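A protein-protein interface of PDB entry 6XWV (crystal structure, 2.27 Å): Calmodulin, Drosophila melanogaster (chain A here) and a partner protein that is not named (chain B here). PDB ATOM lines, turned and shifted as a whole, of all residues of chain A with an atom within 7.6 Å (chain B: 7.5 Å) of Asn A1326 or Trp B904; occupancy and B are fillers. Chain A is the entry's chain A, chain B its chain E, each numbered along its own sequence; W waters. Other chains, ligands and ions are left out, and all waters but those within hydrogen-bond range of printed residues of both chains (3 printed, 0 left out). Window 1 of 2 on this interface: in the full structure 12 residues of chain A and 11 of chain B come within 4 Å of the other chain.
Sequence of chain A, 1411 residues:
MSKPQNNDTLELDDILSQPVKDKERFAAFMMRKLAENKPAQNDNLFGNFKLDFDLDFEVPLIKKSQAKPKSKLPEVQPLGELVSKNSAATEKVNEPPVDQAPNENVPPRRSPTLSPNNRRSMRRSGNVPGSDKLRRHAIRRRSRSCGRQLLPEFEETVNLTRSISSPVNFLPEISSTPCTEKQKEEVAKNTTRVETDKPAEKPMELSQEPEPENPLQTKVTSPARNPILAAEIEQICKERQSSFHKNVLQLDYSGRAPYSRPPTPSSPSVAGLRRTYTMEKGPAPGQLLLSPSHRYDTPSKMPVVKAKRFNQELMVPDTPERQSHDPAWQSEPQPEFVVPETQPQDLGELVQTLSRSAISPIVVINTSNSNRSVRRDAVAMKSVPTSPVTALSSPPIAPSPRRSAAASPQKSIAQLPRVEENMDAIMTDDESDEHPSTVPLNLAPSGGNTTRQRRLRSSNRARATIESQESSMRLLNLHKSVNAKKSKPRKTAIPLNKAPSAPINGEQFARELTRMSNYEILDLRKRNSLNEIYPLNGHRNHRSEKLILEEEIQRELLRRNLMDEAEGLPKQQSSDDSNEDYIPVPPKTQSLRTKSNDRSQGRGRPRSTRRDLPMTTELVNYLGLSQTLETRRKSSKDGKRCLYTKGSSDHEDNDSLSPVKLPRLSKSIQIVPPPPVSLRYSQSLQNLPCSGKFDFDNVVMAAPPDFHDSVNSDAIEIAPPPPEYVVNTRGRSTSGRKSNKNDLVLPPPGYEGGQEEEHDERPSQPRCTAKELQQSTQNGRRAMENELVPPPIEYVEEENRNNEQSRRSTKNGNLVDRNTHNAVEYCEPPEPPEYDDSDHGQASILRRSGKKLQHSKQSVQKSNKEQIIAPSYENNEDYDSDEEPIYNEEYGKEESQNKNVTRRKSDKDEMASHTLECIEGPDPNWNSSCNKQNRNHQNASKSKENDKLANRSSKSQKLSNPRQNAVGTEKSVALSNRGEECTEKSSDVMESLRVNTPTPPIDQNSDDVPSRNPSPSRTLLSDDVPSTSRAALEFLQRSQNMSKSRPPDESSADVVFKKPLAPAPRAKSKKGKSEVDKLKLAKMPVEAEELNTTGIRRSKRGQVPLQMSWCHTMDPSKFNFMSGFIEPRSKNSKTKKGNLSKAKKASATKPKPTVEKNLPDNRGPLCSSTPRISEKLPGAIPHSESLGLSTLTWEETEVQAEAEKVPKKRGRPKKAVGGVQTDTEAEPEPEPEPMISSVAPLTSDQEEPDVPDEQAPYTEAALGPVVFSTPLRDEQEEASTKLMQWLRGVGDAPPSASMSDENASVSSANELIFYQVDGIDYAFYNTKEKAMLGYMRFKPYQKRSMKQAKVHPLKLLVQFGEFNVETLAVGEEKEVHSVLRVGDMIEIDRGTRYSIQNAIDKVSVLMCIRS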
ATOM      1  N   ALA A1304      25.837 -16.491  35.815  1.00  0.00           N
ATOM      2  CA  ALA A1304      24.734 -16.512  34.859  1.00  0.00           C
ATOM      3  C   ALA A1304      25.006 -15.619  33.656  1.00  0.00           C
ATOM      4  O   ALA A1304      24.440 -15.845  32.580  1.00  0.00           O
ATOM      5  CB  ALA A1304      23.436 -16.087  35.541  1.00  0.00           C
ATOM      6  N   SER A1305      25.854 -14.598  33.816  1.00  0.00           N
ATOM      7  CA  SER A1305      26.250 -13.786  32.670  1.00  0.00           C
ATOM      8  C   SER A1305      26.950 -14.617  31.605  1.00  0.00           C
ATOM      9  O   SER A1305      27.011 -14.200  30.443  1.00  0.00           O
ATOM     10  CB  SER A1305      27.167 -12.649  33.128  1.00  0.00           C
ATOM     11  OG  SER A1305      26.423 -11.606  33.725  1.00  0.00           O
ATOM     12  N   VAL A1306      27.463 -15.786  31.977  1.00  0.00           N
ATOM     13  CA  VAL A1306      28.340 -16.589  31.135  1.00  0.00           C
ATOM     14  C   VAL A1306      27.523 -17.677  30.447  1.00  0.00           C
ATOM     15  O   VAL A1306      26.798 -18.435  31.106  1.00  0.00           O
ATOM     16  CB  VAL A1306      29.487 -17.198  31.961  1.00  0.00           C
ATOM     17  CG1 VAL A1306      30.301 -18.160  31.121  1.00  0.00           C
ATOM     18  CG2 VAL A1306      30.375 -16.094  32.544  1.00  0.00           C
ATOM     19  N   SER A1307      27.608 -17.729  29.123  1.00  0.00           N
ATOM     20  CA  SER A1307      27.006 -18.794  28.329  1.00  0.00           C
ATOM     21  C   SER A1307      28.147 -19.580  27.696  1.00  0.00           C
ATOM     22  O   SER A1307      28.710 -19.165  26.679  1.00  0.00           O
ATOM     23  CB  SER A1307      26.054 -18.221  27.286  1.00  0.00           C
ATOM     24  OG  SER A1307      24.903 -17.684  27.917  1.00  0.00           O
ATOM     25  N   SER A1308      28.463 -20.730  28.280  1.00  0.00           N
ATOM     26  CA  SER A1308      29.613 -21.482  27.812  1.00  0.00           C
ATOM     27  C   SER A1308      29.240 -22.325  26.599  1.00  0.00           C
ATOM     28  O   SER A1308      28.064 -22.540  26.293  1.00  0.00           O
ATOM     29  CB  SER A1308      30.168 -22.373  28.926  1.00  0.00           C
ATOM     30  OG  SER A1308      29.703 -23.705  28.795  1.00  0.00           O
ATOM     31  N   GLU A1311      26.567 -25.037  26.383  1.00  0.00           N
ATOM     32  CA  GLU A1311      25.149 -24.776  26.193  1.00  0.00           C
ATOM     33  C   GLU A1311      24.742 -24.860  24.734  1.00  0.00           C
ATOM     34  O   GLU A1311      23.595 -24.536  24.401  1.00  0.00           O
ATOM     35  CB  GLU A1311      24.793 -23.373  26.695  1.00  0.00           C
ATOM     36  CG  GLU A1311      24.780 -23.166  28.195  1.00  0.00           C
ATOM     37  CD  GLU A1311      24.645 -21.694  28.554  1.00  0.00           C
ATOM     38  OE1 GLU A1311      24.350 -20.888  27.646  1.00  0.00           O
ATOM     39  OE2 GLU A1311      24.812 -21.344  29.740  1.00  0.00           O
ATOM     40  N   LEU A1312      25.637 -25.314  23.858  1.00  0.00           N
ATOM     41  CA  LEU A1312      25.310 -25.419  22.442  1.00  0.00           C
ATOM     42  C   LEU A1312      24.763 -26.818  22.188  1.00  0.00           C
ATOM     43  O   LEU A1312      25.449 -27.720  21.705  1.00  0.00           O
ATOM     44  CB  LEU A1312      26.534 -25.114  21.589  1.00  0.00           C
ATOM     45  CG  LEU A1312      27.070 -23.685  21.720  1.00  0.00           C
ATOM     46  CD1 LEU A1312      28.319 -23.489  20.878  1.00  0.00           C
ATOM     47  CD2 LEU A1312      26.000 -22.678  21.353  1.00  0.00           C
ATOM     48  N   ALA A1323      21.512 -24.319  17.176  1.00  0.00           N
ATOM     49  CA  ALA A1323      22.079 -24.301  18.518  1.00  0.00           C
ATOM     50  C   ALA A1323      22.201 -22.858  18.975  1.00  0.00           C
ATOM     51  O   ALA A1323      22.828 -22.039  18.297  1.00  0.00           O
ATOM     52  CB  ALA A1323      23.450 -24.988  18.568  1.00  0.00           C
ATOM     53  N   PHE A1324      21.600 -22.551  20.117  1.00  0.00           N
ATOM     54  CA  PHE A1324      21.603 -21.209  20.678  1.00  0.00           C
ATOM     55  C   PHE A1324      22.284 -21.240  22.038  1.00  0.00           C
ATOM     56  O   PHE A1324      22.205 -22.238  22.762  1.00  0.00           O
ATOM     57  CB  PHE A1324      20.178 -20.656  20.836  1.00  0.00           C
ATOM     58  CG  PHE A1324      19.548 -20.217  19.545  1.00  0.00           C
ATOM     59  CD1 PHE A1324      20.010 -19.094  18.877  1.00  0.00           C
ATOM     60  CD2 PHE A1324      18.493 -20.929  19.001  1.00  0.00           C
ATOM     61  CE1 PHE A1324      19.427 -18.689  17.689  1.00  0.00           C
ATOM     62  CE2 PHE A1324      17.905 -20.532  17.812  1.00  0.00           C
ATOM     63  CZ  PHE A1324      18.372 -19.409  17.154  1.00  0.00           C
ATOM     64  N   TYR A1325      22.967 -20.154  22.385  1.00  0.00           N
ATOM     65  CA  TYR A1325      23.470 -20.035  23.744  1.00  0.00           C
ATOM     66  C   TYR A1325      22.285 -19.719  24.647  1.00  0.00           C
ATOM     67  O   TYR A1325      21.369 -18.990  24.251  1.00  0.00           O
ATOM     68  CB  TYR A1325      24.513 -18.921  23.851  1.00  0.00           C
ATOM     69  CG  TYR A1325      25.837 -19.188  23.160  1.00  0.00           C
ATOM     70  CD1 TYR A1325      26.813 -19.978  23.755  1.00  0.00           C
ATOM     71  CD2 TYR A1325      26.120 -18.622  21.923  1.00  0.00           C
ATOM     72  CE1 TYR A1325      28.029 -20.210  23.128  1.00  0.00           C
ATOM     73  CE2 TYR A1325      27.328 -18.850  21.287  1.00  0.00           C
ATOM     74  CZ  TYR A1325      28.282 -19.645  21.891  1.00  0.00           C
ATOM     75  OH  TYR A1325      29.484 -19.870  21.255  1.00  0.00           O
ATOM     76  N   ASN A1326      22.303 -20.245  25.870  1.00  0.00           N
ATOM     77  CA  ASN A1326      21.234 -19.924  26.814  1.00  0.00           C
ATOM     78  C   ASN A1326      21.607 -18.588  27.441  1.00  0.00           C
ATOM     79  O   ASN A1326      22.433 -18.524  28.352  1.00  0.00           O
ATOM     80  CB  ASN A1326      21.072 -21.033  27.847  1.00  0.00           C
ATOM     81  CG  ASN A1326      19.848 -20.841  28.723  1.00  0.00           C
ATOM     82  OD1 ASN A1326      19.041 -19.940  28.488  1.00  0.00           O
ATOM     83  ND2 ASN A1326      19.696 -21.695  29.730  1.00  0.00           N
ATOM     84  N   THR A1327      20.949 -17.524  27.002  1.00  0.00           N
ATOM     85  CA  THR A1327      21.279 -16.165  27.403  1.00  0.00           C
ATOM     86  C   THR A1327      20.076 -15.468  28.018  1.00  0.00           C
ATOM     87  O   THR A1327      18.942 -15.955  27.959  1.00  0.00           O
ATOM     88  CB  THR A1327      21.798 -15.349  26.217  1.00  0.00           C
ATOM     89  OG1 THR A1327      20.882 -15.470  25.126  1.00  0.00           O
ATOM     90  CG2 THR A1327      23.171 -15.854  25.780  1.00  0.00           C
ATOM     91  N   LYS A1328      20.349 -14.292  28.598  1.00  0.00           N
ATOM     92  CA  LYS A1328      19.302 -13.537  29.279  1.00  0.00           C
ATOM     93  C   LYS A1328      18.122 -13.243  28.345  1.00  0.00           C
ATOM     94  O   LYS A1328      16.978 -13.575  28.670  1.00  0.00           O
ATOM     95  CB  LYS A1328      19.865 -12.245  29.864  1.00  0.00           C
ATOM     96  CG  LYS A1328      19.128 -11.805  31.125  1.00  0.00           C
ATOM     97  CD  LYS A1328      19.880 -10.681  31.829  1.00  0.00           C
ATOM     98  CE  LYS A1328      19.748  -9.383  31.053  1.00  0.00           C
ATOM     99  NZ  LYS A1328      19.094  -8.301  31.829  1.00  0.00           N
ATOM    100  N   GLU A1329      18.353 -12.615  27.177  1.00  0.00           N
ATOM    101  CA  GLU A1329      17.290 -12.638  26.162  1.00  0.00           C
ATOM    102  C   GLU A1329      17.494 -13.867  25.276  1.00  0.00           C
ATOM    103  O   GLU A1329      18.617 -14.149  24.845  1.00  0.00           O
ATOM    104  CB  GLU A1329      17.096 -11.398  25.267  1.00  0.00           C
ATOM    105  CG  GLU A1329      16.900  -9.958  25.847  1.00  0.00           C
ATOM    106  CD  GLU A1329      17.925  -8.939  25.316  1.00  0.00           C
ATOM    107  OE1 GLU A1329      18.485  -9.179  24.230  1.00  0.00           O
ATOM    108  OE2 GLU A1329      18.157  -7.907  25.971  1.00  0.00           O
ATOM    109  N   LYS A1330      16.415 -14.614  25.050  1.00  0.00           N
ATOM    110  CA  LYS A1330      16.497 -15.902  24.375  1.00  0.00           C
ATOM    111  C   LYS A1330      16.853 -15.761  22.897  1.00  0.00           C
ATOM    112  O   LYS A1330      16.413 -14.831  22.218  1.00  0.00           O
ATOM    113  CB  LYS A1330      15.160 -16.625  24.503  1.00  0.00           C
ATOM    114  CG  LYS A1330      14.736 -16.942  25.924  1.00  0.00           C
ATOM    115  CD  LYS A1330      13.454 -17.768  25.966  1.00  0.00           C
ATOM    116  CE  LYS A1330      12.265 -16.943  26.433  1.00  0.00           C
ATOM    117  NZ  LYS A1330      11.042 -17.788  26.580  1.00  0.00           N
ATOM    118  N   ALA A1331      17.649 -16.712  22.402  1.00  0.00           N
ATOM    119  CA  ALA A1331      17.905 -16.903  20.966  1.00  0.00           C
ATOM    120  C   ALA A1331      18.521 -15.682  20.279  1.00  0.00           C
ATOM    121  O   ALA A1331      18.234 -15.399  19.114  1.00  0.00           O
ATOM    122  CB  ALA A1331      16.628 -17.329  20.238  1.00  0.00           C
ATOM    123  N   LEU A1333      21.975 -15.280  20.064  1.00  0.00           N
ATOM    124  CA  LEU A1333      23.238 -15.699  19.465  1.00  0.00           C
ATOM    125  C   LEU A1333      23.225 -17.208  19.293  1.00  0.00           C
ATOM    126  O   LEU A1333      23.047 -17.938  20.274  1.00  0.00           O
ATOM    127  CB  LEU A1333      24.429 -15.265  20.328  1.00  0.00           C
ATOM    128  CG  LEU A1333      25.809 -15.414  19.684  1.00  0.00           C
ATOM    129  CD1 LEU A1333      25.904 -14.553  18.438  1.00  0.00           C
ATOM    130  CD2 LEU A1333      26.914 -15.050  20.668  1.00  0.00           C
ATOM    131  N   GLY B 897      10.565 -23.517  21.192  1.00  0.00           N
ATOM    132  CA  GLY B 897      10.233 -22.401  22.061  1.00  0.00           C
ATOM    133  C   GLY B 897      10.061 -22.819  23.508  1.00  0.00           C
ATOM    134  O   GLY B 897      10.484 -22.108  24.425  1.00  0.00           O
ATOM    135  N   LYS B 898       9.445 -23.982  23.735  1.00  0.00           N
ATOM    136  CA  LYS B 898       9.265 -24.460  25.103  1.00  0.00           C
ATOM    137  C   LYS B 898      10.577 -24.965  25.690  1.00  0.00           C
ATOM    138  O   LYS B 898      10.882 -24.701  26.860  1.00  0.00           O
ATOM    139  CB  LYS B 898       8.204 -25.560  25.145  1.00  0.00           C
ATOM    140  N   ILE B 899      11.363 -25.700  24.898  1.00  0.00           N
ATOM    141  CA  ILE B 899      12.630 -26.230  25.391  1.00  0.00           C
ATOM    142  C   ILE B 899      13.585 -25.093  25.736  1.00  0.00           C
ATOM    143  O   ILE B 899      14.246 -25.116  26.782  1.00  0.00           O
ATOM    144  CB  ILE B 899      13.243 -27.204  24.366  1.00  0.00           C
ATOM    145  CG1 ILE B 899      12.300 -28.386  24.127  1.00  0.00           C
ATOM    146  CG2 ILE B 899      14.603 -27.701  24.844  1.00  0.00           C
ATOM    147  CD1 ILE B 899      11.746 -29.000  25.397  1.00  0.00           C
ATOM    148  N   ILE B 900      13.667 -24.078  24.871  1.00  0.00           N
ATOM    149  CA  ILE B 900      14.453 -22.893  25.203  1.00  0.00           C
ATOM    150  C   ILE B 900      13.860 -22.188  26.415  1.00  0.00           C
ATOM    151  O   ILE B 900      14.590 -21.644  27.253  1.00  0.00           O
ATOM    152  CB  ILE B 900      14.543 -21.951  23.989  1.00  0.00           C
ATOM    153  CG1 ILE B 900      15.283 -22.630  22.835  1.00  0.00           C
ATOM    154  CG2 ILE B 900      15.239 -20.645  24.366  1.00  0.00           C
ATOM    155  CD1 ILE B 900      16.724 -22.977  23.147  1.00  0.00           C
ATOM    156  N   GLY B 901      12.530 -22.194  26.535  1.00  0.00           N
ATOM    157  CA  GLY B 901      11.896 -21.542  27.668  1.00  0.00           C
ATOM    158  C   GLY B 901      12.207 -22.220  28.988  1.00  0.00           C
ATOM    159  O   GLY B 901      12.449 -21.550  29.998  1.00  0.00           O
ATOM    160  N   GLU B 902      12.205 -23.556  29.003  1.00  0.00           N
ATOM    161  CA  GLU B 902      12.552 -24.279  30.224  1.00  0.00           C
ATOM    162  C   GLU B 902      14.018 -24.068  30.586  1.00  0.00           C
ATOM    163  O   GLU B 902      14.347 -23.766  31.739  1.00  0.00           O
ATOM    164  CB  GLU B 902      12.245 -25.768  30.062  1.00  0.00           C
ATOM    165  N   ARG B 903      14.913 -24.226  29.608  1.00  0.00           N
ATOM    166  CA  ARG B 903      16.335 -24.019  29.862  1.00  0.00           C
ATOM    167  C   ARG B 903      16.612 -22.595  30.325  1.00  0.00           C
ATOM    168  O   ARG B 903      17.465 -22.373  31.190  1.00  0.00           O
ATOM    169  CB  ARG B 903      17.145 -24.340  28.605  1.00  0.00           C
ATOM    170  CG  ARG B 903      17.067 -25.796  28.167  1.00  0.00           C
ATOM    171  CD  ARG B 903      17.912 -26.021  26.925  1.00  0.00           C
ATOM    172  NE  ARG B 903      19.281 -25.533  27.098  1.00  0.00           N
ATOM    173  CZ  ARG B 903      20.091 -25.209  26.097  1.00  0.00           C
ATOM    174  NH1 ARG B 903      19.675 -25.315  24.841  1.00  0.00           N
ATOM    175  NH2 ARG B 903      21.314 -24.773  26.351  1.00  0.00           N
ATOM    176  N   TRP B 904      15.904 -21.615  29.761  1.00  0.00           N
ATOM    177  CA  TRP B 904      16.071 -20.239  30.218  1.00  0.00           C
ATOM    178  C   TRP B 904      15.684 -20.099  31.683  1.00  0.00           C
ATOM    179  O   TRP B 904      16.351 -19.388  32.444  1.00  0.00           O
ATOM    180  CB  TRP B 904      15.242 -19.281  29.359  1.00  0.00           C
ATOM    181  CG  TRP B 904      15.300 -17.854  29.839  1.00  0.00           C
ATOM    182  CD1 TRP B 904      16.136 -16.873  29.387  1.00  0.00           C
ATOM    183  CD2 TRP B 904      14.502 -17.253  30.872  1.00  0.00           C
ATOM    184  NE1 TRP B 904      15.905 -15.702  30.068  1.00  0.00           N
ATOM    185  CE2 TRP B 904      14.908 -15.908  30.985  1.00  0.00           C
ATOM    186  CE3 TRP B 904      13.484 -17.721  31.709  1.00  0.00           C
ATOM    187  CZ2 TRP B 904      14.331 -15.027  31.900  1.00  0.00           C
ATOM    188  CZ3 TRP B 904      12.914 -16.845  32.622  1.00  0.00           C
ATOM    189  CH2 TRP B 904      13.339 -15.514  32.708  1.00  0.00           C
ATOM    190  N   ALA B 905      14.602 -20.764  32.095  1.00  0.00           N
ATOM    191  CA  ALA B 905      14.093 -20.577  33.451  1.00  0.00           C
ATOM    192  C   ALA B 905      14.989 -21.249  34.481  1.00  0.00           C
ATOM    193  O   ALA B 905      15.228 -20.693  35.558  1.00  0.00           O
ATOM    194  CB  ALA B 905      12.664 -21.106  33.555  1.00  0.00           C
ATOM    195  N   ARG B 906      15.489 -22.448  34.172  1.00  0.00           N
ATOM    196  CA  ARG B 906      16.338 -23.164  35.114  1.00  0.00           C
ATOM    197  C   ARG B 906      17.632 -22.423  35.402  1.00  0.00           C
ATOM    198  O   ARG B 906      18.285 -22.710  36.412  1.00  0.00           O
ATOM    199  CB  ARG B 906      16.642 -24.565  34.583  1.00  0.00           C
ATOM    200  CG  ARG B 906      15.477 -25.512  34.745  1.00  0.00           C
ATOM    201  CD  ARG B 906      15.779 -26.906  34.232  1.00  0.00           C
ATOM    202  NE  ARG B 906      14.541 -27.632  33.961  1.00  0.00           N
ATOM    203  CZ  ARG B 906      13.703 -28.064  34.900  1.00  0.00           C
ATOM    204  NH1 ARG B 906      13.970 -27.862  36.185  1.00  0.00           N
ATOM    205  NH2 ARG B 906      12.595 -28.708  34.555  1.00  0.00           N
ATOM    206  N   LYS B 907      18.012 -21.474  34.551  1.00  0.00           N
ATOM    207  CA  LYS B 907      19.248 -20.725  34.725  1.00  0.00           C
ATOM    208  C   LYS B 907      19.031 -19.325  35.287  1.00  0.00           C
ATOM    209  O   LYS B 907      19.846 -18.854  36.083  1.00  0.00           O
ATOM    210  CB  LYS B 907      19.990 -20.635  33.384  1.00  0.00           C
ATOM    211  CG  LYS B 907      21.259 -19.807  33.421  1.00  0.00           C
ATOM    212  CD  LYS B 907      22.082 -19.983  32.154  1.00  0.00           C
ATOM    213  CE  LYS B 907      23.256 -19.015  32.130  1.00  0.00           C
ATOM    214  NZ  LYS B 907      23.926 -18.976  30.802  1.00  0.00           N
ATOM    215  N   TYR B 908      17.944 -18.652  34.911  1.00  0.00           N
ATOM    216  CA  TYR B 908      17.794 -17.231  35.196  1.00  0.00           C
ATOM    217  C   TYR B 908      16.667 -16.893  36.164  1.00  0.00           C
ATOM    218  O   TYR B 908      16.568 -15.733  36.585  1.00  0.00           O
ATOM    219  CB  TYR B 908      17.580 -16.454  33.889  1.00  0.00           C
ATOM    220  CG  TYR B 908      18.815 -16.407  33.019  1.00  0.00           C
ATOM    221  CD1 TYR B 908      19.889 -15.595  33.356  1.00  0.00           C
ATOM    222  CD2 TYR B 908      18.908 -17.177  31.865  1.00  0.00           C
ATOM    223  CE1 TYR B 908      21.023 -15.548  32.569  1.00  0.00           C
ATOM    224  CE2 TYR B 908      20.040 -17.135  31.071  1.00  0.00           C
ATOM    225  CZ  TYR B 908      21.094 -16.320  31.430  1.00  0.00           C
ATOM    226  OH  TYR B 908      22.220 -16.274  30.647  1.00  0.00           O
ATOM    227  N   LEU B 909      15.824 -17.857  36.536  1.00  0.00           N
ATOM    228  CA  LEU B 909      14.704 -17.532  37.415  1.00  0.00           C
ATOM    229  C   LEU B 909      15.187 -17.102  38.794  1.00  0.00           C
ATOM    230  O   LEU B 909      14.610 -16.192  39.400  1.00  0.00           O
ATOM    231  CB  LEU B 909      13.747 -18.718  37.527  1.00  0.00           C
ATOM    232  CG  LEU B 909      12.467 -18.578  36.701  1.00  0.00           C
ATOM    233  CD1 LEU B 909      11.429 -19.622  37.101  1.00  0.00           C
ATOM    234  CD2 LEU B 909      11.901 -17.171  36.834  1.00  0.00           C
ATOM    235  N   LYS B 910      16.254 -17.729  39.300  1.00  0.00           N
ATOM    236  CA  LYS B 910      16.730 -17.412  40.644  1.00  0.00           C
ATOM    237  C   LYS B 910      17.202 -15.973  40.781  1.00  0.00           C
ATOM    238  O   LYS B 910      17.384 -15.505  41.911  1.00  0.00           O
ATOM    239  CB  LYS B 910      17.861 -18.362  41.061  1.00  0.00           C
ATOM    240  CG  LYS B 910      19.062 -18.387  40.138  1.00  0.00           C
ATOM    241  CD  LYS B 910      19.993 -19.544  40.485  1.00  0.00           C
ATOM    242  CE  LYS B 910      19.604 -20.820  39.752  1.00  0.00           C
ATOM    243  NZ  LYS B 910      20.796 -21.618  39.344  1.00  0.00           N
ATOM    244  N   HIS B 912      15.400 -13.437  39.437  1.00  0.00           N
ATOM    245  CA  HIS B 912      14.196 -12.623  39.358  1.00  0.00           C
ATOM    246  C   HIS B 912      13.275 -12.836  40.552  1.00  0.00           C
ATOM    247  O   HIS B 912      12.110 -12.427  40.505  1.00  0.00           O
ATOM    248  CB  HIS B 912      13.446 -12.913  38.056  1.00  0.00           C
ATOM    249  CG  HIS B 912      14.183 -12.482  36.826  1.00  0.00           C
ATOM    250  ND1 HIS B 912      14.925 -13.354  36.060  1.00  0.00           N
ATOM    251  CD2 HIS B 912      14.292 -11.271  36.229  1.00  0.00           C
ATOM    252  CE1 HIS B 912      15.460 -12.700  35.044  1.00  0.00           C
ATOM    253  NE2 HIS B 912      15.091 -11.434  35.125  1.00  0.00           N
HETATM  254  O   HOH W   1      10.761 -19.559  24.696  1.00  0.00           O
HETATM  255  O   HOH W   2      24.937 -15.486  28.961  1.00  0.00           O
HETATM  256  O   HOH W   3      21.197 -25.065  22.347  1.00  0.00           O
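Water W2 lies within hydrogen-bond range of the side-chain hydroxyl (OG) of Ser A1307 (2.4 Å), the backbone carbonyl oxygen (O) of Ser A1305 (2.9 Å) and the side-chain hydroxyl (OH) of Tyr B908 (3.3 Å).
Water W1 lies within hydrogen-bond range of the backbone carbonyl oxygen (O) of Gly B897 (2.6 Å) and the side-chain amino group (NZ) of Lys A1330 (2.6 Å).
Water W3 lies within hydrogen-bond range of NH1 of Arg B903, O of Phe A1324 and O of Glu A1311.
OG1 of Thr A1327 is in hydrogen-bond range of O of Glu A1329, at 2.6 Å.
O of Tyr B908 sits at hydrogen-bond distance from ND1 of His B912.
OG of Ser A1307 sits at hydrogen-bond distance from O of Asn A1326, 2.6 Å away.
The side-chain amino group of Lys B907 lies within hydrogen-bond range of the side-chain hydroxyl of Tyr B908.
The side-chain hydroxyl of Ser A1307 sits close to the side-chain carboxylate of Glu A1311.
The side-chain carboxylate (OE1) of Glu A1311 sits at hydrogen-bond distance from the backbone NH (N) of Asn A1326.
Of the 17 printed residues of chain A, 8 touch a printed residue of chain B.
Hydrophobic or aromatic side chains of chain A that line the printed part of chain B: Ala A1304.
Hydrophobic or aromatic side chains of chain B that line the printed part of chain A: Ile B900, Trp B904 and Tyr B908.
Among the printed residues, 16 pairs touch across the chains.
Among the printed residues, Asp or Glu carboxylates within 4 Å of a Lys or Arg side-chain nitrogen of the other chain: Glu A1311 with Lys B907 (2.7 Å).
Asn A1326 touches just these residues of chain B: Arg B903 (2.8 Å), Trp B904 (3.5 Å), Lys B907 (2.9 Å) and Tyr B908 (3.2 Å).
Trp B904 touches just these residues of chain A: Asn A1326, Thr A1327, Lys A1328 and Lys A1330.
Of the printed residues of chain B, Lys A1328 touches Trp B904 (2.8 Å) and Tyr B908 (3.4 Å).
Printed residues of chain A within 4 Å of Lys B907: Ala A1304 (3.4 Å), Val A1306 (2.9 Å), Ser A1307 (3.3 Å), Glu A1311 (2.7 Å) and Asn A1326 (2.9 Å).
Of the printed residues of chain B, Glu A1311 touches Arg B903 and Lys B907.
Tyr A1325 touches none of the printed residues of chain B.
His B912 touches none of the printed residues of chain A.
The nearest residue of chain A that does not touch Trp B904 is Glu A1329 (4.9 Å).
Among the printed residues, pairs that only touch across the chains: Thr A1327 with Trp B904 (3.3 Å), Thr A1327 with Tyr B908 (3.4 Å), Ala A1304 with Lys B907 (3.4 Å), Asn A1326 with Trp B904 (3.5 Å), Lys A1330 with Trp B904 (3.7 Å) and Lys A1330 with Ile B900 (3.7 Å).
O of Ala A1304 sits at hydrogen-bond distance from OH of Tyr B908, at 3.0 Å.
The backbone carbonyl oxygen (O) of Asn A1326 lies within hydrogen-bond range of the side-chain hydroxyl (OH) of Tyr B908 (3.2 Å).
The backbone carbonyl oxygen (O) of Asn A1326 is in hydrogen-bond range of the side-chain amino group (NZ) of Lys B907 (2.9 Å).
NZ of Lys B907 is in hydrogen-bond range of OG of Ser A1307, at 3.3 Å.
The backbone carbonyl oxygen (O) of Lys A1328 sits at hydrogen-bond distance from the indole nitrogen (NE1) of Trp B904, at 2.8 Å.
The backbone NH (N) of Lys A1328 is in hydrogen-bond range of the side-chain hydroxyl (OH) of Tyr B908.
The side-chain amide nitrogen (ND2) of Asn A1326 is in hydrogen-bond range of the backbone carbonyl oxygen (O) of Arg B903 (2.8 Å).
NZ of Lys B907 is in hydrogen-bond range of O of Val A1306 (2.9 Å).
OE2 of Glu A1311 is in salt-bridge range of NZ of Lys B907, 2.7 Å away.
NH2 of Arg B903 sits at hydrogen-bond distance from O of Glu A1311, 3.0 Å away.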
